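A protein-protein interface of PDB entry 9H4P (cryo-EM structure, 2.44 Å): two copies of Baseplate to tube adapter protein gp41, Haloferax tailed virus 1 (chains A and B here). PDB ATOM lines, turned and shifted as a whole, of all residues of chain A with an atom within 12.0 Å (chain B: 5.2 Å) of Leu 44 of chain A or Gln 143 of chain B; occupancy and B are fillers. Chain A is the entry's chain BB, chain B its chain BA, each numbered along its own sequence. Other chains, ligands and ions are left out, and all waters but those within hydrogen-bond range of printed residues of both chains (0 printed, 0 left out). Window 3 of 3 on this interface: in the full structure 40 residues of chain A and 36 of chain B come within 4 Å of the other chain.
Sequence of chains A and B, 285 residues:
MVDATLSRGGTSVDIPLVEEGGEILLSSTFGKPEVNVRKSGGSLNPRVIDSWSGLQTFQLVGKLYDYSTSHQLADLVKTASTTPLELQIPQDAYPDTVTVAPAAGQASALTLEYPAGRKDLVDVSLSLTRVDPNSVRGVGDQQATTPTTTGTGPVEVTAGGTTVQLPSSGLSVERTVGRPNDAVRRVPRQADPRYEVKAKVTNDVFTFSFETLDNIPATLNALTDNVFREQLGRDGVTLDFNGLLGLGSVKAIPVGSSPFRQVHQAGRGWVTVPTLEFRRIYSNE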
ATOM      1  N   VAL A  37     -10.720  16.845  -3.703  1.00  0.00           N
ATOM      2  CA  VAL A  37     -10.372  18.204  -4.102  1.00  0.00           C
ATOM      3  C   VAL A  37      -9.046  18.124  -4.862  1.00  0.00           C
ATOM      4  O   VAL A  37      -8.052  17.649  -4.309  1.00  0.00           O
ATOM      5  CB  VAL A  37     -10.275  19.157  -2.888  1.00  0.00           C
ATOM      6  CG1 VAL A  37      -9.908  20.582  -3.290  1.00  0.00           C
ATOM      7  CG2 VAL A  37     -11.544  19.156  -2.042  1.00  0.00           C
ATOM      8  N   ARG A  38      -9.035  18.584  -6.121  1.00  0.00           N
ATOM      9  CA  ARG A  38      -7.854  18.492  -6.973  1.00  0.00           C
ATOM     10  C   ARG A  38      -6.779  19.455  -6.468  1.00  0.00           C
ATOM     11  O   ARG A  38      -7.073  20.622  -6.201  1.00  0.00           O
ATOM     12  CB  ARG A  38      -8.223  18.782  -8.435  1.00  0.00           C
ATOM     13  CG  ARG A  38      -8.813  17.601  -9.193  1.00  0.00           C
ATOM     14  CD  ARG A  38      -9.928  16.849  -8.480  1.00  0.00           C
ATOM     15  NE  ARG A  38     -10.726  15.973  -9.327  1.00  0.00           N
ATOM     16  CZ  ARG A  38     -10.593  14.652  -9.442  1.00  0.00           C
ATOM     17  NH1 ARG A  38     -11.408  13.990 -10.245  1.00  0.00           N
ATOM     18  NH2 ARG A  38      -9.667  13.994  -8.764  1.00  0.00           N
ATOM     19  N   LYS A  39      -5.534  18.961  -6.357  1.00  0.00           N
ATOM     20  CA  LYS A  39      -4.420  19.727  -5.805  1.00  0.00           C
ATOM     21  C   LYS A  39      -3.928  20.808  -6.776  1.00  0.00           C
ATOM     22  O   LYS A  39      -3.275  21.764  -6.348  1.00  0.00           O
ATOM     23  CB  LYS A  39      -3.288  18.796  -5.354  1.00  0.00           C
ATOM     24  CG  LYS A  39      -3.631  17.905  -4.164  1.00  0.00           C
ATOM     25  CD  LYS A  39      -2.476  17.096  -3.625  1.00  0.00           C
ATOM     26  CE  LYS A  39      -1.475  17.926  -2.852  1.00  0.00           C
ATOM     27  NZ  LYS A  39      -0.399  17.084  -2.289  1.00  0.00           N
ATOM     28  N   SER A  40      -4.256  20.658  -8.072  1.00  0.00           N
ATOM     29  CA  SER A  40      -3.766  21.506  -9.155  1.00  0.00           C
ATOM     30  C   SER A  40      -4.796  21.569 -10.294  1.00  0.00           C
ATOM     31  O   SER A  40      -5.942  21.153 -10.111  1.00  0.00           O
ATOM     32  CB  SER A  40      -2.408  21.013  -9.618  1.00  0.00           C
ATOM     33  OG  SER A  40      -1.745  21.985 -10.414  1.00  0.00           O
ATOM     34  N   GLY A  41      -4.385  22.086 -11.467  1.00  0.00           N
ATOM     35  CA  GLY A  41      -5.276  22.402 -12.581  1.00  0.00           C
ATOM     36  C   GLY A  41      -5.288  23.904 -12.876  1.00  0.00           C
ATOM     37  O   GLY A  41      -4.852  24.691 -12.036  1.00  0.00           O
ATOM     38  N   GLY A  42      -5.828  24.306 -14.040  1.00  0.00           N
ATOM     39  CA  GLY A  42      -5.629  25.648 -14.578  1.00  0.00           C
ATOM     40  C   GLY A  42      -6.642  26.720 -14.152  1.00  0.00           C
ATOM     41  O   GLY A  42      -6.515  27.862 -14.597  1.00  0.00           O
ATOM     42  N   SER A  43      -7.629  26.378 -13.302  1.00  0.00           N
ATOM     43  CA  SER A  43      -8.622  27.326 -12.795  1.00  0.00           C
ATOM     44  C   SER A  43      -8.165  27.937 -11.463  1.00  0.00           C
ATOM     45  O   SER A  43      -7.327  27.338 -10.791  1.00  0.00           O
ATOM     46  CB  SER A  43      -9.976  26.658 -12.663  1.00  0.00           C
ATOM     47  OG  SER A  43      -9.910  25.514 -11.821  1.00  0.00           O
ATOM     48  N   LEU A  44      -8.723  29.100 -11.070  1.00  0.00           N
ATOM     49  CA  LEU A  44      -8.373  29.761  -9.812  1.00  0.00           C
ATOM     50  C   LEU A  44      -8.773  28.922  -8.593  1.00  0.00           C
ATOM     51  O   LEU A  44      -8.052  28.906  -7.594  1.00  0.00           O
ATOM     52  CB  LEU A  44      -9.004  31.159  -9.727  1.00  0.00           C
ATOM     53  CG  LEU A  44      -8.185  32.316 -10.302  1.00  0.00           C
ATOM     54  CD1 LEU A  44      -9.024  33.583 -10.367  1.00  0.00           C
ATOM     55  CD2 LEU A  44      -6.911  32.570  -9.504  1.00  0.00           C
ATOM     56  N   ASN A  45      -9.934  28.258  -8.679  1.00  0.00           N
ATOM     57  CA  ASN A  45     -10.464  27.415  -7.617  1.00  0.00           C
ATOM     58  C   ASN A  45     -10.514  25.972  -8.133  1.00  0.00           C
ATOM     59  O   ASN A  45     -10.698  25.765  -9.337  1.00  0.00           O
ATOM     60  CB  ASN A  45     -11.827  27.929  -7.129  1.00  0.00           C
ATOM     61  CG  ASN A  45     -11.863  29.411  -6.806  1.00  0.00           C
ATOM     62  OD1 ASN A  45     -11.003  29.921  -6.088  1.00  0.00           O
ATOM     63  ND2 ASN A  45     -12.867  30.105  -7.319  1.00  0.00           N
ATOM     64  N   PRO A  46     -10.344  24.935  -7.267  1.00  0.00           N
ATOM     65  CA  PRO A  46     -10.265  23.544  -7.735  1.00  0.00           C
ATOM     66  C   PRO A  46     -11.609  22.937  -8.145  1.00  0.00           C
ATOM     67  O   PRO A  46     -12.658  23.315  -7.616  1.00  0.00           O
ATOM     68  CB  PRO A  46      -9.709  22.796  -6.507  1.00  0.00           C
ATOM     69  CG  PRO A  46     -10.225  23.597  -5.322  1.00  0.00           C
ATOM     70  CD  PRO A  46     -10.209  25.035  -5.799  1.00  0.00           C
ATOM     71  N   ARG A  47     -11.553  21.994  -9.095  1.00  0.00           N
ATOM     72  CA  ARG A  47     -12.646  21.058  -9.312  1.00  0.00           C
ATOM     73  C   ARG A  47     -12.632  20.023  -8.189  1.00  0.00           C
ATOM     74  O   ARG A  47     -11.575  19.725  -7.628  1.00  0.00           O
ATOM     75  CB  ARG A  47     -12.541  20.392 -10.686  1.00  0.00           C
ATOM     76  CG  ARG A  47     -13.271  21.158 -11.781  1.00  0.00           C
ATOM     77  CD  ARG A  47     -13.274  20.433 -13.114  1.00  0.00           C
ATOM     78  NE  ARG A  47     -14.360  20.885 -13.979  1.00  0.00           N
ATOM     79  CZ  ARG A  47     -14.293  21.864 -14.886  1.00  0.00           C
ATOM     80  NH1 ARG A  47     -15.364  22.163 -15.603  1.00  0.00           N
ATOM     81  NH2 ARG A  47     -13.172  22.538 -15.081  1.00  0.00           N
ATOM     82  N   VAL A  48     -13.822  19.487  -7.875  1.00  0.00           N
ATOM     83  CA  VAL A  48     -14.031  18.554  -6.774  1.00  0.00           C
ATOM     84  C   VAL A  48     -14.961  17.423  -7.226  1.00  0.00           C
ATOM     85  O   VAL A  48     -15.651  17.547  -8.239  1.00  0.00           O
ATOM     86  CB  VAL A  48     -14.580  19.258  -5.510  1.00  0.00           C
ATOM     87  CG1 VAL A  48     -13.650  20.337  -4.964  1.00  0.00           C
ATOM     88  CG2 VAL A  48     -16.005  19.790  -5.674  1.00  0.00           C
ATOM     89  N   ASP B  75      -8.345  39.771  -3.084  1.00  0.00           N
ATOM     90  CA  ASP B  75      -8.242  39.664  -4.535  1.00  0.00           C
ATOM     91  C   ASP B  75      -6.821  39.968  -5.017  1.00  0.00           C
ATOM     92  O   ASP B  75      -6.365  39.350  -5.979  1.00  0.00           O
ATOM     93  CB  ASP B  75      -9.281  40.543  -5.241  1.00  0.00           C
ATOM     94  CG  ASP B  75     -10.724  40.128  -5.005  1.00  0.00           C
ATOM     95  OD1 ASP B  75     -10.945  39.019  -4.483  1.00  0.00           O
ATOM     96  OD2 ASP B  75     -11.616  40.916  -5.357  1.00  0.00           O
ATOM     97  N   LYS B  78      -4.646  36.883  -3.997  1.00  0.00           N
ATOM     98  CA  LYS B  78      -4.985  35.636  -4.679  1.00  0.00           C
ATOM     99  C   LYS B  78      -4.661  35.670  -6.179  1.00  0.00           C
ATOM    100  O   LYS B  78      -4.409  34.613  -6.763  1.00  0.00           O
ATOM    101  CB  LYS B  78      -6.424  35.188  -4.402  1.00  0.00           C
ATOM    102  CG  LYS B  78      -6.634  33.681  -4.540  1.00  0.00           C
ATOM    103  CD  LYS B  78      -8.032  33.207  -4.222  1.00  0.00           C
ATOM    104  CE  LYS B  78      -9.011  33.459  -5.354  1.00  0.00           C
ATOM    105  NZ  LYS B  78     -10.247  32.656  -5.201  1.00  0.00           N
ATOM    106  N   THR B  79      -4.679  36.868  -6.792  1.00  0.00           N
ATOM    107  CA  THR B  79      -4.481  37.075  -8.225  1.00  0.00           C
ATOM    108  C   THR B  79      -3.127  36.524  -8.683  1.00  0.00           C
ATOM    109  O   THR B  79      -2.112  36.755  -8.021  1.00  0.00           O
ATOM    110  CB  THR B  79      -4.591  38.575  -8.550  1.00  0.00           C
ATOM    111  OG1 THR B  79      -5.966  38.951  -8.463  1.00  0.00           O
ATOM    112  CG2 THR B  79      -4.069  38.974  -9.915  1.00  0.00           C
ATOM    113  N   ALA B  80      -3.121  35.822  -9.828  1.00  0.00           N
ATOM    114  CA  ALA B  80      -1.889  35.469 -10.524  1.00  0.00           C
ATOM    115  C   ALA B  80      -1.554  36.553 -11.551  1.00  0.00           C
ATOM    116  O   ALA B  80      -2.372  36.843 -12.424  1.00  0.00           O
ATOM    117  CB  ALA B  80      -2.028  34.110 -11.180  1.00  0.00           C
ATOM    118  N   ASP B 141      -1.936  35.384 -16.684  1.00  0.00           N
ATOM    119  CA  ASP B 141      -2.560  36.302 -15.739  1.00  0.00           C
ATOM    120  C   ASP B 141      -3.966  35.790 -15.415  1.00  0.00           C
ATOM    121  O   ASP B 141      -4.719  35.443 -16.327  1.00  0.00           O
ATOM    122  CB  ASP B 141      -2.641  37.727 -16.305  1.00  0.00           C
ATOM    123  CG  ASP B 141      -1.311  38.423 -16.524  1.00  0.00           C
ATOM    124  OD1 ASP B 141      -0.722  38.875 -15.538  1.00  0.00           O
ATOM    125  OD2 ASP B 141      -0.889  38.521 -17.685  1.00  0.00           O
ATOM    126  N   GLN B 142      -4.306  35.741 -14.117  1.00  0.00           N
ATOM    127  CA  GLN B 142      -5.640  35.392 -13.644  1.00  0.00           C
ATOM    128  C   GLN B 142      -6.043  36.358 -12.530  1.00  0.00           C
ATOM    129  O   GLN B 142      -5.614  36.209 -11.384  1.00  0.00           O
ATOM    130  CB  GLN B 142      -5.704  33.935 -13.173  1.00  0.00           C
ATOM    131  CG  GLN B 142      -5.614  32.914 -14.302  1.00  0.00           C
ATOM    132  CD  GLN B 142      -5.830  31.485 -13.866  1.00  0.00           C
ATOM    133  OE1 GLN B 142      -5.471  31.084 -12.759  1.00  0.00           O
ATOM    134  NE2 GLN B 142      -6.409  30.693 -14.751  1.00  0.00           N
ATOM    135  N   GLN B 143      -6.863  37.351 -12.896  1.00  0.00           N
ATOM    136  CA  GLN B 143      -7.438  38.297 -11.953  1.00  0.00           C
ATOM    137  C   GLN B 143      -8.469  37.574 -11.084  1.00  0.00           C
ATOM    138  O   GLN B 143      -9.475  37.082 -11.597  1.00  0.00           O
ATOM    139  CB  GLN B 143      -8.058  39.475 -12.714  1.00  0.00           C
ATOM    140  CG  GLN B 143      -8.747  40.509 -11.828  1.00  0.00           C
ATOM    141  CD  GLN B 143      -7.807  41.188 -10.862  1.00  0.00           C
ATOM    142  OE1 GLN B 143      -6.772  41.730 -11.241  1.00  0.00           O
ATOM    143  NE2 GLN B 143      -8.176  41.181  -9.594  1.00  0.00           N
ATOM    144  N   ALA B 144      -8.200  37.510  -9.773  1.00  0.00           N
ATOM    145  CA  ALA B 144      -9.151  36.981  -8.805  1.00  0.00           C
ATOM    146  C   ALA B 144     -10.234  38.020  -8.515  1.00  0.00           C
ATOM    147  O   ALA B 144      -9.969  39.223  -8.572  1.00  0.00           O
ATOM    148  CB  ALA B 144      -8.429  36.566  -7.547  1.00  0.00           C
ATOM    149  N   THR B 145     -11.448  37.537  -8.202  1.00  0.00           N
ATOM    150  CA  THR B 145     -12.561  38.393  -7.810  1.00  0.00           C
ATOM    151  C   THR B 145     -13.307  37.793  -6.619  1.00  0.00           C
ATOM    152  O   THR B 145     -13.532  36.584  -6.556  1.00  0.00           O
ATOM    153  CB  THR B 145     -13.536  38.661  -8.968  1.00  0.00           C
ATOM    154  OG1 THR B 145     -14.082  37.421  -9.419  1.00  0.00           O
ATOM    155  CG2 THR B 145     -12.926  39.405 -10.135  1.00  0.00           C
ATOM    156  N   ARG B 179      -1.622  30.907  -2.185  1.00  0.00           N
ATOM    157  CA  ARG B 179      -1.198  30.484  -3.511  1.00  0.00           C
ATOM    158  C   ARG B 179      -0.163  29.360  -3.383  1.00  0.00           C
ATOM    159  O   ARG B 179       1.005  29.560  -3.728  1.00  0.00           O
ATOM    160  CB  ARG B 179      -0.664  31.694  -4.290  1.00  0.00           C
ATOM    161  CG  ARG B 179      -1.705  32.758  -4.628  1.00  0.00           C
ATOM    162  CD  ARG B 179      -1.211  33.759  -5.660  1.00  0.00           C
ATOM    163  NE  ARG B 179      -0.664  33.041  -6.808  1.00  0.00           N
ATOM    164  CZ  ARG B 179      -1.363  32.562  -7.839  1.00  0.00           C
ATOM    165  NH1 ARG B 179      -0.734  31.916  -8.806  1.00  0.00           N
ATOM    166  NH2 ARG B 179      -2.670  32.748  -7.923  1.00  0.00           N
ATOM    167  N   LYS B 200      -2.769  28.587 -11.831  1.00  0.00           N
ATOM    168  CA  LYS B 200      -3.181  27.292 -11.296  1.00  0.00           C
ATOM    169  C   LYS B 200      -3.964  27.478  -9.994  1.00  0.00           C
ATOM    170  O   LYS B 200      -3.949  28.567  -9.415  1.00  0.00           O
ATOM    171  CB  LYS B 200      -1.961  26.393 -11.057  1.00  0.00           C
ATOM    172  CG  LYS B 200      -1.264  25.900 -12.316  1.00  0.00           C
ATOM    173  CD  LYS B 200      -0.082  25.009 -12.031  1.00  0.00           C
ATOM    174  CE  LYS B 200       0.684  24.687 -13.295  1.00  0.00           C
ATOM    175  NZ  LYS B 200       1.862  23.830 -13.031  1.00  0.00           N
ATOM    176  N   VAL B 201      -4.623  26.394  -9.541  1.00  0.00           N
ATOM    177  CA  VAL B 201      -5.487  26.308  -8.364  1.00  0.00           C
ATOM    178  C   VAL B 201      -4.873  26.998  -7.138  1.00  0.00           C
ATOM    179  O   VAL B 201      -3.719  26.744  -6.787  1.00  0.00           O
ATOM    180  CB  VAL B 201      -5.859  24.833  -8.072  1.00  0.00           C
ATOM    181  CG1 VAL B 201      -6.351  24.587  -6.645  1.00  0.00           C
ATOM    182  CG2 VAL B 201      -6.855  24.279  -9.087  1.00  0.00           C
ATOM    183  N   THR B 202      -5.695  27.833  -6.478  1.00  0.00           N
ATOM    184  CA  THR B 202      -5.360  28.538  -5.246  1.00  0.00           C
ATOM    185  C   THR B 202      -6.172  27.964  -4.081  1.00  0.00           C
ATOM    186  O   THR B 202      -7.034  27.105  -4.287  1.00  0.00           O
ATOM    187  CB  THR B 202      -5.593  30.053  -5.391  1.00  0.00           C
ATOM    188  OG1 THR B 202      -6.988  30.316  -5.561  1.00  0.00           O
ATOM    189  CG2 THR B 202      -4.822  30.672  -6.538  1.00  0.00           C
ATOM    190  N   ASN B 284     -15.497  30.198 -12.024  1.00  0.00           N
ATOM    191  CA  ASN B 284     -15.224  31.261 -12.987  1.00  0.00           C
ATOM    192  C   ASN B 284     -15.356  30.757 -14.429  1.00  0.00           C
ATOM    193  O   ASN B 284     -15.240  29.557 -14.683  1.00  0.00           O
ATOM    194  CB  ASN B 284     -13.854  31.902 -12.735  1.00  0.00           C
ATOM    195  CG  ASN B 284     -13.766  32.671 -11.434  1.00  0.00           C
ATOM    196  OD1 ASN B 284     -14.053  32.137 -10.364  1.00  0.00           O
ATOM    197  ND2 ASN B 284     -13.354  33.926 -11.515  1.00  0.00           N
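NZ of Lys 78 of chain B sits at hydrogen-bond distance from OD1 of Asn 45 of chain A, at 3.0 Å. O of Gly 42 of chain A sits at hydrogen-bond distance from NE2 of Gln 142 of chain B. N of Val 201 of chain B sits at hydrogen-bond distance from O of Gly 41 of chain A, at 3.0 Å. The backbone carbonyl oxygen (O) of Ser 43 of chain A lies within hydrogen-bond range of the backbone NH (N) of Val 201 of chain B (3.1 Å). The side-chain hydroxyl (OG1) of Thr 202 of chain B lies within hydrogen-bond range of the backbone carbonyl oxygen (O) of Leu 44 of chain A, at 2.7 Å.
The backbone carbonyl oxygen (O) of Lys 78 of chain B lies within hydrogen-bond range of the guanidinium group (NH2) of Arg 179 of chain B, 2.8 Å away. The side-chain amide nitrogen (NE2) of Gln 143 of chain B is in hydrogen-bond range of the side-chain hydroxyl (OG1) of Thr 79 of chain B (3.3 Å). The backbone NH (N) of Ala 144 of chain B lies within hydrogen-bond range of the side-chain hydroxyl (OG1) of Thr 79 of chain B, 3.0 Å away. The backbone carbonyl oxygen (O) of Ala 80 of chain B is in hydrogen-bond range of the backbone NH (N) of Gln 142 of chain B. O of Asn 45 of chain A lies within hydrogen-bond range of OG of Ser 43 of chain A (2.6 Å).
Ser 40 of chain A touches Lys 200 of chain B (OG to CD, 3.8 Å). O of Ser 40 of chain A touches CG2 of Val 201 of chain B, at 3.4 Å. CA of Lys 200 of chain B touches O of Gly 41 of chain A, at 3.2 Å. C of Lys 200 of chain B touches O of Ser 43 of chain A, 3.5 Å away. Leu 44 of chain A touches Gln 142 of chain B (CD2 to OE1, 3.9 Å). Gln 143 of chain B touches Leu 44 of chain A (O to CD1, 3.7 Å). Ala 144 of chain B touches Leu 44 of chain A (CA to CD1, 3.7 Å). Val 201 of chain B touches Leu 44 of chain A (CA to O, 3.7 Å). Asn 45 of chain A touches Asn 284 of chain B. Pro 46 of chain A touches Val 201 of chain B (CA to CG2, 3.7 Å).
Of chain B, only Gln 142, Gln 143, Ala 144, Val 201 and Thr 202 come within 4 Å of Leu 44 of chain A. Gln 143 of chain B touches one residue of chain A. No residue of chain A comes within 4 Å of Asp 75 of chain B. Thr 79 of chain B touches none of the printed residues of chain A. No residue of chain A comes within 4 Å of Asp 141 of chain B. Gln 142 of chain B touches two residues of chain A. Ala 144 of chain B touches just one residue of chain A: Leu 44 (3.7 Å). Printed residues of chain A within 4 Å of Val 201 of chain B: Ser 40, Gly 41, Ser 43, Leu 44 and Pro 46. Of chain A, only Asn 45 (3.8 Å) comes within 4 Å of Asn 284 of chain B. Of the printed residues of chain B, Asn 45 of chain A touches Lys 78 (3.0 Å) and Asn 284 (3.8 Å). Of the printed residues of chain B, Gly 42 of chain A touches Gln 142. Of the printed residues of chain B, Gly 41 of chain A touches Lys 200 and Val 201. Printed residues of chain B within 4 Å of Ser 40 of chain A: Lys 200 (3.8 Å) and Val 201 (3.4 Å). Printed residues of chain B within 4 Å of Pro 46 of chain A: Val 201. The nearest residue of chain B that does not touch Leu 44 of chain A is Lys 78 of chain B (4.2 Å).
Hydrophobic or aromatic side chains of chain B that line the printed part of chain A: Val 201. Of the 12 printed residues of chain A, 7 touch a printed residue of chain B. Hydrophobic or aromatic side chains of chain A that line the printed part of chain B: Leu 44 and Pro 46. Among the printed residues, 15 pairs touch across the chains.
No position is printed for both chains. Of the 15 pairs that touch across the chains among the printed residues, none has its exchanged pair printed and touching as well.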
